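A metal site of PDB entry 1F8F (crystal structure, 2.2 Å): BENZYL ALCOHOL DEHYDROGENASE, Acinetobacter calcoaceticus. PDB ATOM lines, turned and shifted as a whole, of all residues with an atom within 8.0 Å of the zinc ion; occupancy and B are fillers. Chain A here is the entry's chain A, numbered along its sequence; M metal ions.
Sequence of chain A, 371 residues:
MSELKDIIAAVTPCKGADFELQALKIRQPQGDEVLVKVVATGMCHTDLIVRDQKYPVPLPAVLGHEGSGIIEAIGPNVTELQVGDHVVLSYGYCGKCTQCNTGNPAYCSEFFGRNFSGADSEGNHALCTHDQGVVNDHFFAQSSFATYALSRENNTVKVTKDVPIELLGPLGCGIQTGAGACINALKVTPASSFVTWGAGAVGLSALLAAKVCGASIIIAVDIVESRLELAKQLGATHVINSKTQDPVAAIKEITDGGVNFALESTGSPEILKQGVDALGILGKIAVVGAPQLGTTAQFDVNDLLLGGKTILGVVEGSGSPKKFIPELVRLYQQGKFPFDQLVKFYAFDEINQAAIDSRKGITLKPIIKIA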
ATOM      1  N   GLY A  92       4.836  18.919 -24.656  1.00  0.00           N
ATOM      2  CA  GLY A  92       6.228  18.712 -24.422  1.00  0.00           C
ATOM      3  C   GLY A  92       7.252  19.572 -25.138  1.00  0.00           C
ATOM      4  O   GLY A  92       7.391  19.644 -26.351  1.00  0.00           O
ATOM      5  N   TYR A  93       8.000  20.342 -24.315  1.00  0.00           N
ATOM      6  CA  TYR A  93       9.048  21.240 -24.792  1.00  0.00           C
ATOM      7  C   TYR A  93      10.350  21.170 -23.997  1.00  0.00           C
ATOM      8  O   TYR A  93      10.410  20.803 -22.817  1.00  0.00           O
ATOM      9  CB  TYR A  93       8.571  22.678 -24.945  1.00  0.00           C
ATOM     10  CG  TYR A  93       8.197  23.441 -23.710  1.00  0.00           C
ATOM     11  CD1 TYR A  93       7.019  23.116 -23.019  1.00  0.00           C
ATOM     12  CD2 TYR A  93       8.952  24.483 -23.190  1.00  0.00           C
ATOM     13  CE1 TYR A  93       6.600  23.768 -21.876  1.00  0.00           C
ATOM     14  CE2 TYR A  93       8.565  25.169 -22.060  1.00  0.00           C
ATOM     15  CZ  TYR A  93       7.396  24.799 -21.415  1.00  0.00           C
ATOM     16  OH  TYR A  93       7.023  25.470 -20.261  1.00  0.00           O
ATOM     17  N   CYS A  94      11.458  21.486 -24.672  1.00  0.00           N
ATOM     18  CA  CYS A  94      12.790  21.424 -24.078  1.00  0.00           C
ATOM     19  C   CYS A  94      13.140  22.628 -23.196  1.00  0.00           C
ATOM     20  O   CYS A  94      13.787  22.277 -22.206  1.00  0.00           O
ATOM     21  CB  CYS A  94      13.878  21.171 -25.123  1.00  0.00           C
ATOM     22  SG  CYS A  94      14.573  22.691 -25.818  1.00  0.00           S
ATOM     23  N   GLY A  95      12.761  23.855 -23.574  1.00  0.00           N
ATOM     24  CA  GLY A  95      12.989  25.045 -22.769  1.00  0.00           C
ATOM     25  C   GLY A  95      14.411  25.560 -22.653  1.00  0.00           C
ATOM     26  O   GLY A  95      14.760  26.418 -21.822  1.00  0.00           O
ATOM     27  N   LYS A  96      15.268  25.080 -23.554  1.00  0.00           N
ATOM     28  CA  LYS A  96      16.673  25.458 -23.599  1.00  0.00           C
ATOM     29  C   LYS A  96      17.058  25.852 -25.037  1.00  0.00           C
ATOM     30  O   LYS A  96      18.124  26.471 -25.182  1.00  0.00           O
ATOM     31  CB  LYS A  96      17.541  24.234 -23.243  1.00  0.00           C
ATOM     32  CG  LYS A  96      17.428  23.602 -21.900  1.00  0.00           C
ATOM     33  CD  LYS A  96      18.549  22.612 -21.588  1.00  0.00           C
ATOM     34  CE  LYS A  96      18.153  21.612 -20.488  1.00  0.00           C
ATOM     35  NZ  LYS A  96      19.277  20.691 -20.143  1.00  0.00           N
ATOM     36  N   CYS A  97      16.277  25.534 -26.069  1.00  0.00           N
ATOM     37  CA  CYS A  97      16.668  25.893 -27.433  1.00  0.00           C
ATOM     38  C   CYS A  97      16.346  27.354 -27.797  1.00  0.00           C
ATOM     39  O   CYS A  97      15.805  28.083 -26.945  1.00  0.00           O
ATOM     40  CB  CYS A  97      16.033  24.948 -28.462  1.00  0.00           C
ATOM     41  SG  CYS A  97      14.224  25.210 -28.666  1.00  0.00           S
ATOM     42  N   THR A  98      16.637  27.769 -29.043  1.00  0.00           N
ATOM     43  CA  THR A  98      16.411  29.173 -29.437  1.00  0.00           C
ATOM     44  C   THR A  98      14.922  29.580 -29.323  1.00  0.00           C
ATOM     45  O   THR A  98      14.545  30.679 -28.859  1.00  0.00           O
ATOM     46  CB  THR A  98      16.902  29.396 -30.899  1.00  0.00           C
ATOM     47  OG1 THR A  98      18.325  29.307 -30.970  1.00  0.00           O
ATOM     48  CG2 THR A  98      16.453  30.725 -31.467  1.00  0.00           C
ATOM     49  N   GLN A  99      14.045  28.692 -29.812  1.00  0.00           N
ATOM     50  CA  GLN A  99      12.591  28.970 -29.742  1.00  0.00           C
ATOM     51  C   GLN A  99      12.101  28.950 -28.305  1.00  0.00           C
ATOM     52  O   GLN A  99      11.426  29.920 -27.981  1.00  0.00           O
ATOM     53  CB  GLN A  99      11.837  28.092 -30.715  1.00  0.00           C
ATOM     54  CG  GLN A  99      11.843  28.735 -32.094  1.00  0.00           C
ATOM     55  CD  GLN A  99      13.104  28.403 -32.832  1.00  0.00           C
ATOM     56  OE1 GLN A  99      13.673  29.264 -33.526  1.00  0.00           O
ATOM     57  NE2 GLN A  99      13.538  27.160 -32.682  1.00  0.00           N
ATOM     58  N   CYS A 100      12.472  28.046 -27.412  1.00  0.00           N
ATOM     59  CA  CYS A 100      12.061  28.062 -26.033  1.00  0.00           C
ATOM     60  C   CYS A 100      12.576  29.278 -25.296  1.00  0.00           C
ATOM     61  O   CYS A 100      11.711  29.967 -24.733  1.00  0.00           O
ATOM     62  CB  CYS A 100      12.407  26.757 -25.315  1.00  0.00           C
ATOM     63  SG  CYS A 100      11.652  25.255 -26.047  1.00  0.00           S
ATOM     64  N   ASN A 101      13.848  29.727 -25.511  1.00  0.00           N
ATOM     65  CA  ASN A 101      14.384  30.890 -24.871  1.00  0.00           C
ATOM     66  C   ASN A 101      13.793  32.229 -25.334  1.00  0.00           C
ATOM     67  O   ASN A 101      14.060  33.202 -24.618  1.00  0.00           O
ATOM     68  CB  ASN A 101      15.906  31.035 -25.181  1.00  0.00           C
ATOM     69  CG  ASN A 101      16.632  29.827 -24.642  1.00  0.00           C
ATOM     70  OD1 ASN A 101      16.065  29.220 -23.682  1.00  0.00           O
ATOM     71  ND2 ASN A 101      17.786  29.420 -25.178  1.00  0.00           N
ATOM     72  N   ASN A 104       8.586  31.062 -27.430  1.00  0.00           N
ATOM     73  CA  ASN A 104       7.889  30.280 -28.441  1.00  0.00           C
ATOM     74  C   ASN A 104       8.066  28.780 -28.238  1.00  0.00           C
ATOM     75  O   ASN A 104       8.529  28.114 -29.168  1.00  0.00           O
ATOM     76  CB  ASN A 104       8.526  30.590 -29.818  1.00  0.00           C
ATOM     77  CG  ASN A 104       8.502  32.031 -30.265  1.00  0.00           C
ATOM     78  OD1 ASN A 104       7.466  32.596 -30.664  1.00  0.00           O
ATOM     79  ND2 ASN A 104       9.639  32.750 -30.244  1.00  0.00           N
ATOM     80  N   PRO A 105       7.655  28.219 -27.114  1.00  0.00           N
ATOM     81  CA  PRO A 105       7.871  26.790 -26.848  1.00  0.00           C
ATOM     82  C   PRO A 105       7.163  25.889 -27.827  1.00  0.00           C
ATOM     83  O   PRO A 105       7.554  24.761 -28.197  1.00  0.00           O
ATOM     84  CB  PRO A 105       7.382  26.584 -25.402  1.00  0.00           C
ATOM     85  CG  PRO A 105       6.388  27.707 -25.215  1.00  0.00           C
ATOM     86  CD  PRO A 105       7.015  28.908 -25.954  1.00  0.00           C
ATOM     87  N   ALA A 106       6.002  26.380 -28.358  1.00  0.00           N
ATOM     88  CA  ALA A 106       5.302  25.545 -29.345  1.00  0.00           C
ATOM     89  C   ALA A 106       6.201  25.242 -30.555  1.00  0.00           C
ATOM     90  O   ALA A 106       5.856  24.278 -31.243  1.00  0.00           O
ATOM     91  CB  ALA A 106       4.018  26.206 -29.790  1.00  0.00           C
ATOM     92  N   TYR A 107       7.225  26.014 -30.862  1.00  0.00           N
ATOM     93  CA  TYR A 107       8.125  25.925 -31.994  1.00  0.00           C
ATOM     94  C   TYR A 107       9.464  25.323 -31.649  1.00  0.00           C
ATOM     95  O   TYR A 107      10.430  25.315 -32.411  1.00  0.00           O
ATOM     96  CB  TYR A 107       8.159  27.315 -32.749  1.00  0.00           C
ATOM     97  CG  TYR A 107       6.710  27.624 -33.148  1.00  0.00           C
ATOM     98  CD1 TYR A 107       6.025  26.857 -34.077  1.00  0.00           C
ATOM     99  CD2 TYR A 107       6.006  28.609 -32.491  1.00  0.00           C
ATOM    100  CE1 TYR A 107       4.699  27.055 -34.365  1.00  0.00           C
ATOM    101  CE2 TYR A 107       4.690  28.880 -32.851  1.00  0.00           C
ATOM    102  CZ  TYR A 107       4.013  28.068 -33.755  1.00  0.00           C
ATOM    103  OH  TYR A 107       2.703  28.436 -33.997  1.00  0.00           O
ATOM    104  N   CYS A 108       9.588  24.796 -30.435  1.00  0.00           N
ATOM    105  CA  CYS A 108      10.771  24.114 -29.898  1.00  0.00           C
ATOM    106  C   CYS A 108      11.372  23.256 -30.984  1.00  0.00           C
ATOM    107  O   CYS A 108      10.744  22.429 -31.662  1.00  0.00           O
ATOM    108  CB  CYS A 108      10.470  23.221 -28.674  1.00  0.00           C
ATOM    109  SG  CYS A 108      11.707  22.148 -27.936  1.00  0.00           S
ATOM    110  N   SER A 109      12.698  23.342 -31.137  1.00  0.00           N
ATOM    111  CA  SER A 109      13.366  22.515 -32.160  1.00  0.00           C
ATOM    112  C   SER A 109      13.313  21.038 -31.796  1.00  0.00           C
ATOM    113  O   SER A 109      13.651  20.150 -32.591  1.00  0.00           O
ATOM    114  CB  SER A 109      14.755  23.073 -32.471  1.00  0.00           C
ATOM    115  OG  SER A 109      15.593  22.945 -31.326  1.00  0.00           O
ATOM    116  N   GLU A 110      12.823  20.648 -30.613  1.00  0.00           N
ATOM    117  CA  GLU A 110      12.635  19.227 -30.333  1.00  0.00           C
ATOM    118  C   GLU A 110      11.136  18.935 -30.342  1.00  0.00           C
ATOM    119  O   GLU A 110      10.778  17.886 -29.814  1.00  0.00           O
ATOM    120  CB  GLU A 110      13.314  18.835 -29.017  1.00  0.00           C
ATOM    121  CG  GLU A 110      14.744  19.251 -28.823  1.00  0.00           C
ATOM    122  CD  GLU A 110      15.640  18.754 -27.727  1.00  0.00           C
ATOM    123  OE1 GLU A 110      15.347  18.245 -26.617  1.00  0.00           O
ATOM    124  OE2 GLU A 110      16.894  18.893 -27.923  1.00  0.00           O
ATOM    125  N   PHE A 111      10.247  19.746 -30.892  1.00  0.00           N
ATOM    126  CA  PHE A 111       8.822  19.409 -30.852  1.00  0.00           C
ATOM    127  C   PHE A 111       8.545  18.023 -31.370  1.00  0.00           C
ATOM    128  O   PHE A 111       8.309  17.237 -30.452  1.00  0.00           O
ATOM    129  CB  PHE A 111       7.898  20.435 -31.526  1.00  0.00           C
ATOM    130  CG  PHE A 111       6.465  20.363 -31.043  1.00  0.00           C
ATOM    131  CD1 PHE A 111       5.585  19.427 -31.555  1.00  0.00           C
ATOM    132  CD2 PHE A 111       6.013  21.202 -30.026  1.00  0.00           C
ATOM    133  CE1 PHE A 111       4.273  19.378 -31.089  1.00  0.00           C
ATOM    134  CE2 PHE A 111       4.738  21.150 -29.552  1.00  0.00           C
ATOM    135  CZ  PHE A 111       3.850  20.237 -30.099  1.00  0.00           C
ATOM    136  N   ARG A 114       9.704  15.090 -28.496  1.00  0.00           N
ATOM    137  CA  ARG A 114       9.241  15.058 -27.126  1.00  0.00           C
ATOM    138  C   ARG A 114       7.805  14.589 -26.985  1.00  0.00           C
ATOM    139  O   ARG A 114       7.487  14.100 -25.900  1.00  0.00           O
ATOM    140  CB  ARG A 114       9.398  16.436 -26.437  1.00  0.00           C
ATOM    141  CG  ARG A 114      10.826  16.609 -25.940  1.00  0.00           C
ATOM    142  CD  ARG A 114      11.258  18.024 -25.609  1.00  0.00           C
ATOM    143  NE  ARG A 114      12.714  18.085 -25.409  1.00  0.00           N
ATOM    144  CZ  ARG A 114      13.311  17.654 -24.314  1.00  0.00           C
ATOM    145  NH1 ARG A 114      12.508  17.177 -23.365  1.00  0.00           N
ATOM    146  NH2 ARG A 114      14.601  17.666 -24.033  1.00  0.00           N
ATOM    147  N   ASN A 154       8.334  21.699 -16.563  1.00  0.00           N
ATOM    148  CA  ASN A 154       7.890  22.762 -17.486  1.00  0.00           C
ATOM    149  C   ASN A 154       6.574  22.423 -18.212  1.00  0.00           C
ATOM    150  O   ASN A 154       5.928  23.383 -18.665  1.00  0.00           O
ATOM    151  CB  ASN A 154       8.931  23.270 -18.465  1.00  0.00           C
ATOM    152  CG  ASN A 154       9.327  22.254 -19.495  1.00  0.00           C
ATOM    153  OD1 ASN A 154       8.865  21.099 -19.429  1.00  0.00           O
ATOM    154  ND2 ASN A 154      10.176  22.699 -20.427  1.00  0.00           N
HETATM  155 ZN    ZN M   1      13.085  23.843 -27.108  1.00  0.00          ZN
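The zinc ion is bound by SG of Cys 100 (2.3 Å), SG of Cys 94 (2.3 Å), SG of Cys 108 (2.3 Å) and SG of Cys 97 (2.4 Å).
The backbone NH of Gly 95 lies close to the side-chain sulfur of Cys 100.
O of Cys 97 sits at hydrogen-bond distance from ND2 of Asn 101, at 3.0 Å.
SG of Cys 108 lies close to N of Glu 110 (3.3 Å).
The side-chain sulfur (SG) of Cys 97 sits close to the backbone NH (N) of Gln 99 (3.7 Å).
The backbone NH of Lys 96 sits close to the side-chain sulfur of Cys 94 (3.4 Å).
The side-chain sulfur (SG) of Cys 97 lies close to the backbone NH (N) of Ser 109, 3.5 Å away.
N of Gly 95 touches the zinc ion, 3.5 Å away.
Of the 20 residues printed, 5 come within 4 Å of the zinc ion.
The nearest printed residue that does not touch the zinc ion is Ser 109 (4.1 Å).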
